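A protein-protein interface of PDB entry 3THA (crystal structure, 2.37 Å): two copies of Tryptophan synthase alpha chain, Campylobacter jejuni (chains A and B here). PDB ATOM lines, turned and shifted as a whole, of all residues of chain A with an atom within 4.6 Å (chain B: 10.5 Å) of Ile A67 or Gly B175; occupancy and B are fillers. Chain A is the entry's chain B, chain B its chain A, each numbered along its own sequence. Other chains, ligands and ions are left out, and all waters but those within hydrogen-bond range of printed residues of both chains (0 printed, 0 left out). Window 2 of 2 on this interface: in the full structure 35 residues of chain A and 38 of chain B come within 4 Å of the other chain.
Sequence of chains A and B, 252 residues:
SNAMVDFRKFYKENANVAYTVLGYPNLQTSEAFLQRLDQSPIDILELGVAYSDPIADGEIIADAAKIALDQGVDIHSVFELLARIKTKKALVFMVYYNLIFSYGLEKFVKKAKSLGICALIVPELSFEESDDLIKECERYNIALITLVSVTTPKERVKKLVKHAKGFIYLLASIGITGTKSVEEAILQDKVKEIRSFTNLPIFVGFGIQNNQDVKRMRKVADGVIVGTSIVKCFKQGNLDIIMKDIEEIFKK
Among the printed residues, pairs that only touch across the chains: Asp A63 with Gly B175 (3.9 Å), Asp A63 with Phe B206 (3.3 Å), Lys A66 with Ala B172 (2.9 Å), Lys A66 with Ser B173 (3.6 Å), Lys A66 with Phe B206 (3.3 Å), Ile A67 with Gly B175 (3.0 Å), Asp A70 with Thr B151 (3.3 Å) and Asp A70 with Ile B176 (2.9 Å).
The backbone NH (N) of Gly B175 sits at hydrogen-bond distance from the side-chain carboxylate (OE2) of Glu B183 (3.1 Å). OE2 of Glu B183 is in hydrogen-bond range of N of Ile B176 (2.8 Å). O of Ile A67 lies close to OD2 of Asp A70, at 2.7 Å. N of Ala B172 lies within hydrogen-bond range of O of Gly B205. OG1 of Thr B151 sits at hydrogen-bond distance from OG of Ser B149 (3.0 Å).
No position is printed for both chains.
Of chain A, only Asp A63 (3.9 Å) and Ile A67 (3.0 Å) come within 4 Å of Gly B175. Of chain B, only Gly B175 (3.9 Å) and Phe B206 (3.3 Å) come within 4 Å of Asp A63. No residue of chain B comes within 4 Å of Ala A64. No residue of chain B comes within 4 Å of Ala A68. Of the printed residues of chain B, Asp A70 touches Thr B151 (3.3 Å) and Ile B176 (2.9 Å). No residue of chain B comes within 4 Å of Gln A71. Printed residues of chain A within 4 Å of Thr B151: Asp A70 (3.3 Å). Printed residues of chain A within 4 Å of Ser B173: Lys A66 (3.6 Å). Printed residues of chain A within 4 Å of Phe B206: Asp A63 (3.3 Å) and Lys A66 (3.3 Å). Leu B187 touches none of the printed residues of chain A.
Hydrophobic or aromatic side chains of chain B within 4 Å of the printed part of chain A: Ile B176 and Phe B206. Along chain B the printed residues that touch a printed residue of chain A span positions 151 to 206. Hydrophobic or aromatic side chains of chain A that line the printed part of chain B: Ile A67. Among the printed residues, 8 pairs touch across the chains.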
ATOM      1  N   GLY A  23      -2.525  12.164  19.391  1.00  0.00           N
ATOM      2  CA  GLY A  23      -1.471  11.146  19.207  1.00  0.00           C
ATOM      3  C   GLY A  23      -1.828  10.036  18.223  1.00  0.00           C
ATOM      4  O   GLY A  23      -1.077   9.092  18.067  1.00  0.00           O
ATOM      5  N   TYR A  24      -2.968  10.163  17.557  1.00  0.00           N
ATOM      6  CA  TYR A  24      -3.429   9.171  16.637  1.00  0.00           C
ATOM      7  C   TYR A  24      -3.559   9.735  15.202  1.00  0.00           C
ATOM      8  O   TYR A  24      -4.345  10.664  14.989  1.00  0.00           O
ATOM      9  CB  TYR A  24      -4.794   8.635  17.100  1.00  0.00           C
ATOM     10  CG  TYR A  24      -5.383   7.670  16.095  1.00  0.00           C
ATOM     11  CD1 TYR A  24      -4.735   6.470  15.806  1.00  0.00           C
ATOM     12  CD2 TYR A  24      -6.559   7.970  15.393  1.00  0.00           C
ATOM     13  CE1 TYR A  24      -5.265   5.565  14.868  1.00  0.00           C
ATOM     14  CE2 TYR A  24      -7.075   7.077  14.441  1.00  0.00           C
ATOM     15  CZ  TYR A  24      -6.437   5.882  14.200  1.00  0.00           C
ATOM     16  OH  TYR A  24      -6.929   4.985  13.266  1.00  0.00           O
ATOM     17  N   PRO A  25      -2.842   9.157  14.215  1.00  0.00           N
ATOM     18  CA  PRO A  25      -1.979   7.993  14.280  1.00  0.00           C
ATOM     19  C   PRO A  25      -0.584   8.313  14.797  1.00  0.00           C
ATOM     20  O   PRO A  25       0.229   7.383  14.983  1.00  0.00           O
ATOM     21  CB  PRO A  25      -1.904   7.515  12.821  1.00  0.00           C
ATOM     22  CG  PRO A  25      -2.505   8.632  11.985  1.00  0.00           C
ATOM     23  CD  PRO A  25      -2.766   9.794  12.890  1.00  0.00           C
ATOM     24  N   ASP A  63      -8.269   1.401  19.842  1.00  0.00           N
ATOM     25  CA  ASP A  63      -7.150   1.378  18.897  1.00  0.00           C
ATOM     26  C   ASP A  63      -6.348   2.689  18.860  1.00  0.00           C
ATOM     27  O   ASP A  63      -5.102   2.666  19.027  1.00  0.00           O
ATOM     28  CB  ASP A  63      -7.632   0.938  17.535  1.00  0.00           C
ATOM     29  CG  ASP A  63      -7.619  -0.594  17.391  1.00  0.00           C
ATOM     30  OD1 ASP A  63      -6.522  -1.203  17.212  1.00  0.00           O
ATOM     31  OD2 ASP A  63      -8.722  -1.192  17.477  1.00  0.00           O
ATOM     32  N   ALA A  64      -7.054   3.818  18.721  1.00  0.00           N
ATOM     33  CA  ALA A  64      -6.411   5.141  18.620  1.00  0.00           C
ATOM     34  C   ALA A  64      -5.546   5.398  19.853  1.00  0.00           C
ATOM     35  O   ALA A  64      -4.366   5.902  19.753  1.00  0.00           O
ATOM     36  CB  ALA A  64      -7.448   6.217  18.506  1.00  0.00           C
ATOM     37  N   ALA A  65      -6.132   5.032  21.005  1.00  0.00           N
ATOM     38  CA  ALA A  65      -5.503   5.247  22.300  1.00  0.00           C
ATOM     39  C   ALA A  65      -4.304   4.309  22.561  1.00  0.00           C
ATOM     40  O   ALA A  65      -3.293   4.751  23.127  1.00  0.00           O
ATOM     41  CB  ALA A  65      -6.554   5.181  23.442  1.00  0.00           C
ATOM     42  N   LYS A  66      -4.377   3.046  22.103  1.00  0.00           N
ATOM     43  CA  LYS A  66      -3.227   2.161  22.212  1.00  0.00           C
ATOM     44  C   LYS A  66      -2.147   2.723  21.334  1.00  0.00           C
ATOM     45  O   LYS A  66      -0.962   2.792  21.713  1.00  0.00           O
ATOM     46  CB  LYS A  66      -3.522   0.710  21.789  1.00  0.00           C
ATOM     47  CG  LYS A  66      -4.811   0.082  22.336  1.00  0.00           C
ATOM     48  CD  LYS A  66      -4.564  -1.405  22.477  1.00  0.00           C
ATOM     49  CE  LYS A  66      -5.803  -2.210  22.874  1.00  0.00           C
ATOM     50  NZ  LYS A  66      -6.724  -1.649  23.944  1.00  0.00           N
ATOM     51  N   ILE A  67      -2.552   3.144  20.143  1.00  0.00           N
ATOM     52  CA  ILE A  67      -1.582   3.710  19.215  1.00  0.00           C
ATOM     53  C   ILE A  67      -0.907   4.916  19.836  1.00  0.00           C
ATOM     54  O   ILE A  67       0.319   5.000  19.823  1.00  0.00           O
ATOM     55  CB  ILE A  67      -2.184   4.027  17.854  1.00  0.00           C
ATOM     56  CG1 ILE A  67      -2.585   2.708  17.153  1.00  0.00           C
ATOM     57  CG2 ILE A  67      -1.142   4.718  16.995  1.00  0.00           C
ATOM     58  CD1 ILE A  67      -3.793   2.789  16.195  1.00  0.00           C
ATOM     59  N   ALA A  68      -1.686   5.831  20.424  1.00  0.00           N
ATOM     60  CA  ALA A  68      -1.090   6.989  21.037  1.00  0.00           C
ATOM     61  C   ALA A  68      -0.121   6.520  22.121  1.00  0.00           C
ATOM     62  O   ALA A  68       1.029   7.028  22.197  1.00  0.00           O
ATOM     63  CB  ALA A  68      -2.160   7.886  21.642  1.00  0.00           C
ATOM     64  N   LEU A  69      -0.585   5.560  22.942  1.00  0.00           N
ATOM     65  CA  LEU A  69       0.166   5.121  24.129  1.00  0.00           C
ATOM     66  C   LEU A  69       1.499   4.485  23.791  1.00  0.00           C
ATOM     67  O   LEU A  69       2.523   4.850  24.374  1.00  0.00           O
ATOM     68  CB  LEU A  69      -0.640   4.178  25.046  1.00  0.00           C
ATOM     69  CG  LEU A  69      -1.769   4.801  25.855  1.00  0.00           C
ATOM     70  CD1 LEU A  69      -2.624   3.660  26.438  1.00  0.00           C
ATOM     71  CD2 LEU A  69      -1.243   5.744  26.936  1.00  0.00           C
ATOM     72  N   ASP A  70       1.519   3.559  22.849  1.00  0.00           N
ATOM     73  CA  ASP A  70       2.805   2.933  22.498  1.00  0.00           C
ATOM     74  C   ASP A  70       3.729   3.867  21.685  1.00  0.00           C
ATOM     75  O   ASP A  70       4.932   3.622  21.554  1.00  0.00           O
ATOM     76  CB  ASP A  70       2.589   1.645  21.727  1.00  0.00           C
ATOM     77  CG  ASP A  70       2.612   1.868  20.255  1.00  0.00           C
ATOM     78  OD1 ASP A  70       3.375   1.153  19.566  1.00  0.00           O
ATOM     79  OD2 ASP A  70       1.888   2.783  19.795  1.00  0.00           O
ATOM     80  N   GLN A  71       3.125   4.920  21.137  1.00  0.00           N
ATOM     81  CA  GLN A  71       3.779   5.917  20.355  1.00  0.00           C
ATOM     82  C   GLN A  71       4.377   6.902  21.393  1.00  0.00           C
ATOM     83  O   GLN A  71       5.235   7.745  21.072  1.00  0.00           O
ATOM     84  CB  GLN A  71       2.692   6.519  19.472  1.00  0.00           C
ATOM     85  CG  GLN A  71       3.040   7.597  18.538  1.00  0.00           C
ATOM     86  CD  GLN A  71       3.760   7.141  17.281  1.00  0.00           C
ATOM     87  OE1 GLN A  71       3.467   6.098  16.687  1.00  0.00           O
ATOM     88  NE2 GLN A  71       4.695   7.947  16.859  1.00  0.00           N
ATOM     89  N   SER B 149      -1.543  -4.047  29.835  1.00  0.00           N
ATOM     90  CA  SER B 149      -1.510  -3.894  28.393  1.00  0.00           C
ATOM     91  C   SER B 149      -0.123  -4.190  27.795  1.00  0.00           C
ATOM     92  O   SER B 149       0.861  -4.262  28.520  1.00  0.00           O
ATOM     93  CB  SER B 149      -1.912  -2.469  28.059  1.00  0.00           C
ATOM     94  OG  SER B 149      -1.861  -2.266  26.655  1.00  0.00           O
ATOM     95  N   VAL B 150      -0.039  -4.349  26.466  1.00  0.00           N
ATOM     96  CA  VAL B 150       1.236  -4.554  25.801  1.00  0.00           C
ATOM     97  C   VAL B 150       2.055  -3.261  25.833  1.00  0.00           C
ATOM     98  O   VAL B 150       3.273  -3.279  25.635  1.00  0.00           O
ATOM     99  CB  VAL B 150       1.082  -5.114  24.343  1.00  0.00           C
ATOM    100  CG1 VAL B 150       0.300  -6.415  24.343  1.00  0.00           C
ATOM    101  CG2 VAL B 150       0.423  -4.093  23.390  1.00  0.00           C
ATOM    102  N   THR B 151       1.379  -2.145  26.110  1.00  0.00           N
ATOM    103  CA  THR B 151       2.027  -0.825  26.189  1.00  0.00           C
ATOM    104  C   THR B 151       2.457  -0.460  27.613  1.00  0.00           C
ATOM    105  O   THR B 151       3.131   0.546  27.826  1.00  0.00           O
ATOM    106  CB  THR B 151       1.100   0.300  25.649  1.00  0.00           C
ATOM    107  OG1 THR B 151      -0.192   0.224  26.282  1.00  0.00           O
ATOM    108  CG2 THR B 151       0.944   0.176  24.164  1.00  0.00           C
ATOM    109  N   LEU B 171      -4.325  -6.865  27.852  1.00  0.00           N
ATOM    110  CA  LEU B 171      -4.842  -6.229  26.626  1.00  0.00           C
ATOM    111  C   LEU B 171      -3.907  -6.336  25.447  1.00  0.00           C
ATOM    112  O   LEU B 171      -2.771  -5.889  25.520  1.00  0.00           O
ATOM    113  CB  LEU B 171      -5.105  -4.760  26.851  1.00  0.00           C
ATOM    114  CG  LEU B 171      -6.228  -4.614  27.859  1.00  0.00           C
ATOM    115  CD1 LEU B 171      -6.256  -3.181  28.420  1.00  0.00           C
ATOM    116  CD2 LEU B 171      -7.595  -5.062  27.175  1.00  0.00           C
ATOM    117  N   ALA B 172      -4.383  -6.922  24.359  1.00  0.00           N
ATOM    118  CA  ALA B 172      -3.587  -6.982  23.154  1.00  0.00           C
ATOM    119  C   ALA B 172      -3.664  -5.669  22.368  1.00  0.00           C
ATOM    120  O   ALA B 172      -4.330  -4.728  22.792  1.00  0.00           O
ATOM    121  CB  ALA B 172      -4.007  -8.148  22.296  1.00  0.00           C
ATOM    122  N   SER B 173      -2.911  -5.613  21.273  1.00  0.00           N
ATOM    123  CA  SER B 173      -3.099  -4.649  20.205  1.00  0.00           C
ATOM    124  C   SER B 173      -3.476  -5.376  18.914  1.00  0.00           C
ATOM    125  O   SER B 173      -3.196  -6.579  18.759  1.00  0.00           O
ATOM    126  CB  SER B 173      -1.817  -3.867  19.969  1.00  0.00           C
ATOM    127  OG  SER B 173      -1.632  -2.976  21.043  1.00  0.00           O
ATOM    128  N   ILE B 174      -4.119  -4.641  18.000  1.00  0.00           N
ATOM    129  CA  ILE B 174      -4.306  -5.072  16.581  1.00  0.00           C
ATOM    130  C   ILE B 174      -3.509  -4.116  15.655  1.00  0.00           C
ATOM    131  O   ILE B 174      -3.203  -4.436  14.477  1.00  0.00           O
ATOM    132  CB  ILE B 174      -5.844  -5.172  16.160  1.00  0.00           C
ATOM    133  CG1 ILE B 174      -6.640  -6.135  17.077  1.00  0.00           C
ATOM    134  CG2 ILE B 174      -6.015  -5.500  14.645  1.00  0.00           C
ATOM    135  CD1 ILE B 174      -6.455  -7.644  16.810  1.00  0.00           C
ATOM    136  N   GLY B 175      -3.150  -2.953  16.206  1.00  0.00           N
ATOM    137  CA  GLY B 175      -2.414  -1.951  15.438  1.00  0.00           C
ATOM    138  C   GLY B 175      -1.326  -1.145  16.129  1.00  0.00           C
ATOM    139  O   GLY B 175      -1.426   0.082  16.199  1.00  0.00           O
ATOM    140  N   ILE B 176      -0.278  -1.807  16.624  1.00  0.00           N
ATOM    141  CA  ILE B 176       0.961  -1.084  16.958  1.00  0.00           C
ATOM    142  C   ILE B 176       1.833  -0.918  15.704  1.00  0.00           C
ATOM    143  O   ILE B 176       2.469   0.125  15.502  1.00  0.00           O
ATOM    144  CB  ILE B 176       1.765  -1.740  18.126  1.00  0.00           C
ATOM    145  CG1 ILE B 176       1.101  -1.411  19.482  1.00  0.00           C
ATOM    146  CG2 ILE B 176       3.264  -1.327  18.058  1.00  0.00           C
ATOM    147  CD1 ILE B 176       1.947  -1.749  20.725  1.00  0.00           C
ATOM    148  N   THR B 177       1.839  -1.945  14.856  1.00  0.00           N
ATOM    149  CA  THR B 177       2.660  -1.933  13.652  1.00  0.00           C
ATOM    150  C   THR B 177       1.804  -1.754  12.412  1.00  0.00           C
ATOM    151  O   THR B 177       2.254  -1.203  11.395  1.00  0.00           O
ATOM    152  CB  THR B 177       3.406  -3.270  13.475  1.00  0.00           C
ATOM    153  OG1 THR B 177       3.744  -3.815  14.757  1.00  0.00           O
ATOM    154  CG2 THR B 177       4.681  -3.082  12.609  1.00  0.00           C
ATOM    155  N   GLY B 178       0.566  -2.230  12.513  1.00  0.00           N
ATOM    156  CA  GLY B 178      -0.247  -2.531  11.346  1.00  0.00           C
ATOM    157  C   GLY B 178      -0.055  -3.998  10.990  1.00  0.00           C
ATOM    158  O   GLY B 178      -1.032  -4.716  10.754  1.00  0.00           O
ATOM    159  N   THR B 179       1.211  -4.435  10.967  1.00  0.00           N
ATOM    160  CA  THR B 179       1.616  -5.837  10.698  1.00  0.00           C
ATOM    161  C   THR B 179       1.203  -6.789  11.836  1.00  0.00           C
ATOM    162  O   THR B 179       0.862  -6.329  12.942  1.00  0.00           O
ATOM    163  CB  THR B 179       3.128  -5.925  10.496  1.00  0.00           C
ATOM    164  OG1 THR B 179       3.542  -4.812   9.711  1.00  0.00           O
ATOM    165  CG2 THR B 179       3.531  -7.227   9.821  1.00  0.00           C
ATOM    166  N   LYS B 180       1.241  -8.100  11.555  1.00  0.00           N
ATOM    167  CA  LYS B 180       0.686  -9.119  12.458  1.00  0.00           C
ATOM    168  C   LYS B 180       1.686 -10.204  12.850  1.00  0.00           C
ATOM    169  O   LYS B 180       1.649 -10.717  13.970  1.00  0.00           O
ATOM    170  CB  LYS B 180      -0.591  -9.740  11.871  1.00  0.00           C
ATOM    171  CG  LYS B 180      -1.915  -9.162  12.422  1.00  0.00           C
ATOM    172  CD  LYS B 180      -2.248  -7.775  11.852  1.00  0.00           C
ATOM    173  CE  LYS B 180      -3.579  -7.228  12.387  1.00  0.00           C
ATOM    174  NZ  LYS B 180      -4.804  -7.989  11.977  1.00  0.00           N
ATOM    175  N   SER B 181       2.575 -10.553  11.935  1.00  0.00           N
ATOM    176  CA  SER B 181       3.615 -11.515  12.239  1.00  0.00           C
ATOM    177  C   SER B 181       4.322 -11.027  13.505  1.00  0.00           C
ATOM    178  O   SER B 181       4.590 -11.781  14.451  1.00  0.00           O
ATOM    179  CB  SER B 181       4.599 -11.565  11.078  1.00  0.00           C
ATOM    180  OG  SER B 181       3.968 -11.139   9.883  1.00  0.00           O
ATOM    181  N   VAL B 182       4.577  -9.728  13.524  1.00  0.00           N
ATOM    182  CA  VAL B 182       5.452  -9.120  14.510  1.00  0.00           C
ATOM    183  C   VAL B 182       4.676  -8.864  15.784  1.00  0.00           C
ATOM    184  O   VAL B 182       5.179  -9.053  16.894  1.00  0.00           O
ATOM    185  CB  VAL B 182       6.032  -7.779  13.956  1.00  0.00           C
ATOM    186  CG1 VAL B 182       4.904  -6.760  13.709  1.00  0.00           C
ATOM    187  CG2 VAL B 182       7.075  -7.206  14.887  1.00  0.00           C
ATOM    188  N   GLU B 183       3.437  -8.439  15.591  1.00  0.00           N
ATOM    189  CA  GLU B 183       2.591  -7.973  16.666  1.00  0.00           C
ATOM    190  C   GLU B 183       2.166  -9.072  17.646  1.00  0.00           C
ATOM    191  O   GLU B 183       1.697  -8.784  18.736  1.00  0.00           O
ATOM    192  CB  GLU B 183       1.387  -7.286  16.072  1.00  0.00           C
ATOM    193  CG  GLU B 183       0.598  -6.546  17.084  1.00  0.00           C
ATOM    194  CD  GLU B 183      -0.445  -5.685  16.454  1.00  0.00           C
ATOM    195  OE1 GLU B 183      -1.020  -6.095  15.419  1.00  0.00           O
ATOM    196  OE2 GLU B 183      -0.682  -4.591  16.999  1.00  0.00           O
ATOM    197  N   GLU B 184       2.370 -10.320  17.242  1.00  0.00           N
ATOM    198  CA  GLU B 184       2.077 -11.488  18.056  1.00  0.00           C
ATOM    199  C   GLU B 184       3.300 -11.809  18.899  1.00  0.00           C
ATOM    200  O   GLU B 184       3.171 -12.241  20.060  1.00  0.00           O
ATOM    201  CB  GLU B 184       1.758 -12.689  17.157  1.00  0.00           C
ATOM    202  CG  GLU B 184       0.373 -12.664  16.520  1.00  0.00           C
ATOM    203  CD  GLU B 184       0.145 -13.872  15.606  1.00  0.00           C
ATOM    204  OE1 GLU B 184       0.625 -13.880  14.446  1.00  0.00           O
ATOM    205  OE2 GLU B 184      -0.529 -14.819  16.071  1.00  0.00           O
ATOM    206  N   ILE B 186       5.392  -9.521  19.798  1.00  0.00           N
ATOM    207  CA  ILE B 186       5.341  -8.456  20.817  1.00  0.00           C
ATOM    208  C   ILE B 186       4.463  -8.884  21.988  1.00  0.00           C
ATOM    209  O   ILE B 186       4.721  -8.546  23.145  1.00  0.00           O
ATOM    210  CB  ILE B 186       4.847  -7.101  20.229  1.00  0.00           C
ATOM    211  CG1 ILE B 186       5.861  -6.548  19.219  1.00  0.00           C
ATOM    212  CG2 ILE B 186       4.618  -6.069  21.336  1.00  0.00           C
ATOM    213  CD1 ILE B 186       5.312  -5.434  18.319  1.00  0.00           C
ATOM    214  N   LEU B 187       3.436  -9.661  21.678  1.00  0.00           N
ATOM    215  CA  LEU B 187       2.438 -10.101  22.682  1.00  0.00           C
ATOM    216  C   LEU B 187       2.988 -11.239  23.547  1.00  0.00           C
ATOM    217  O   LEU B 187       2.805 -11.263  24.772  1.00  0.00           O
ATOM    218  CB  LEU B 187       1.164 -10.556  21.952  1.00  0.00           C
ATOM    219  CG  LEU B 187      -0.010 -11.014  22.780  1.00  0.00           C
ATOM    220  CD1 LEU B 187      -0.395  -9.926  23.745  1.00  0.00           C
ATOM    221  CD2 LEU B 187      -1.157 -11.414  21.873  1.00  0.00           C
ATOM    222  N   GLY B 205      -7.297 -10.436  25.924  1.00  0.00           N
ATOM    223  CA  GLY B 205      -8.498  -9.943  25.278  1.00  0.00           C
ATOM    224  C   GLY B 205      -8.197  -8.718  24.421  1.00  0.00           C
ATOM    225  O   GLY B 205      -7.025  -8.281  24.332  1.00  0.00           O
ATOM    226  N   PHE B 206      -9.264  -8.143  23.837  1.00  0.00           N
ATOM    227  CA  PHE B 206      -9.219  -7.052  22.851  1.00  0.00           C
ATOM    228  C   PHE B 206      -8.821  -7.567  21.492  1.00  0.00           C
ATOM    229  O   PHE B 206      -7.738  -8.099  21.347  1.00  0.00           O
ATOM    230  CB  PHE B 206      -8.275  -5.902  23.245  1.00  0.00           C
ATOM    231  CG  PHE B 206      -8.313  -4.774  22.281  1.00  0.00           C
ATOM    232  CD1 PHE B 206      -8.949  -3.611  22.602  1.00  0.00           C
ATOM    233  CD2 PHE B 206      -7.720  -4.896  21.019  1.00  0.00           C
ATOM    234  CE1 PHE B 206      -9.016  -2.572  21.667  1.00  0.00           C
ATOM    235  CE2 PHE B 206      -7.780  -3.890  20.102  1.00  0.00           C
ATOM    236  CZ  PHE B 206      -8.416  -2.717  20.431  1.00  0.00           C
ATOM    237  N   GLY B 207      -9.686  -7.406  20.492  1.00  0.00           N
ATOM    238  CA  GLY B 207      -9.342  -7.792  19.106  1.00  0.00           C
ATOM    239  C   GLY B 207      -9.719  -9.203  18.674  1.00  0.00           C
ATOM    240  O   GLY B 207      -9.528  -9.579  17.521  1.00  0.00           O
ATOM    241  N   MET B 217      -5.090 -17.343  19.699  1.00  0.00           N
ATOM    242  CA  MET B 217      -4.851 -16.663  20.945  1.00  0.00           C
ATOM    243  C   MET B 217      -4.618 -17.677  22.015  1.00  0.00           C
ATOM    244  O   MET B 217      -3.933 -17.397  22.995  1.00  0.00           O
ATOM    245  CB  MET B 217      -6.037 -15.773  21.283  1.00  0.00           C
ATOM    246  CG  MET B 217      -5.938 -14.391  20.657  1.00  0.00           C
ATOM    247  SD  MET B 217      -4.248 -13.520  21.143  1.00  0.00           S
ATOM    248  CE  MET B 217      -4.439 -11.882  20.072  1.00  0.00           C
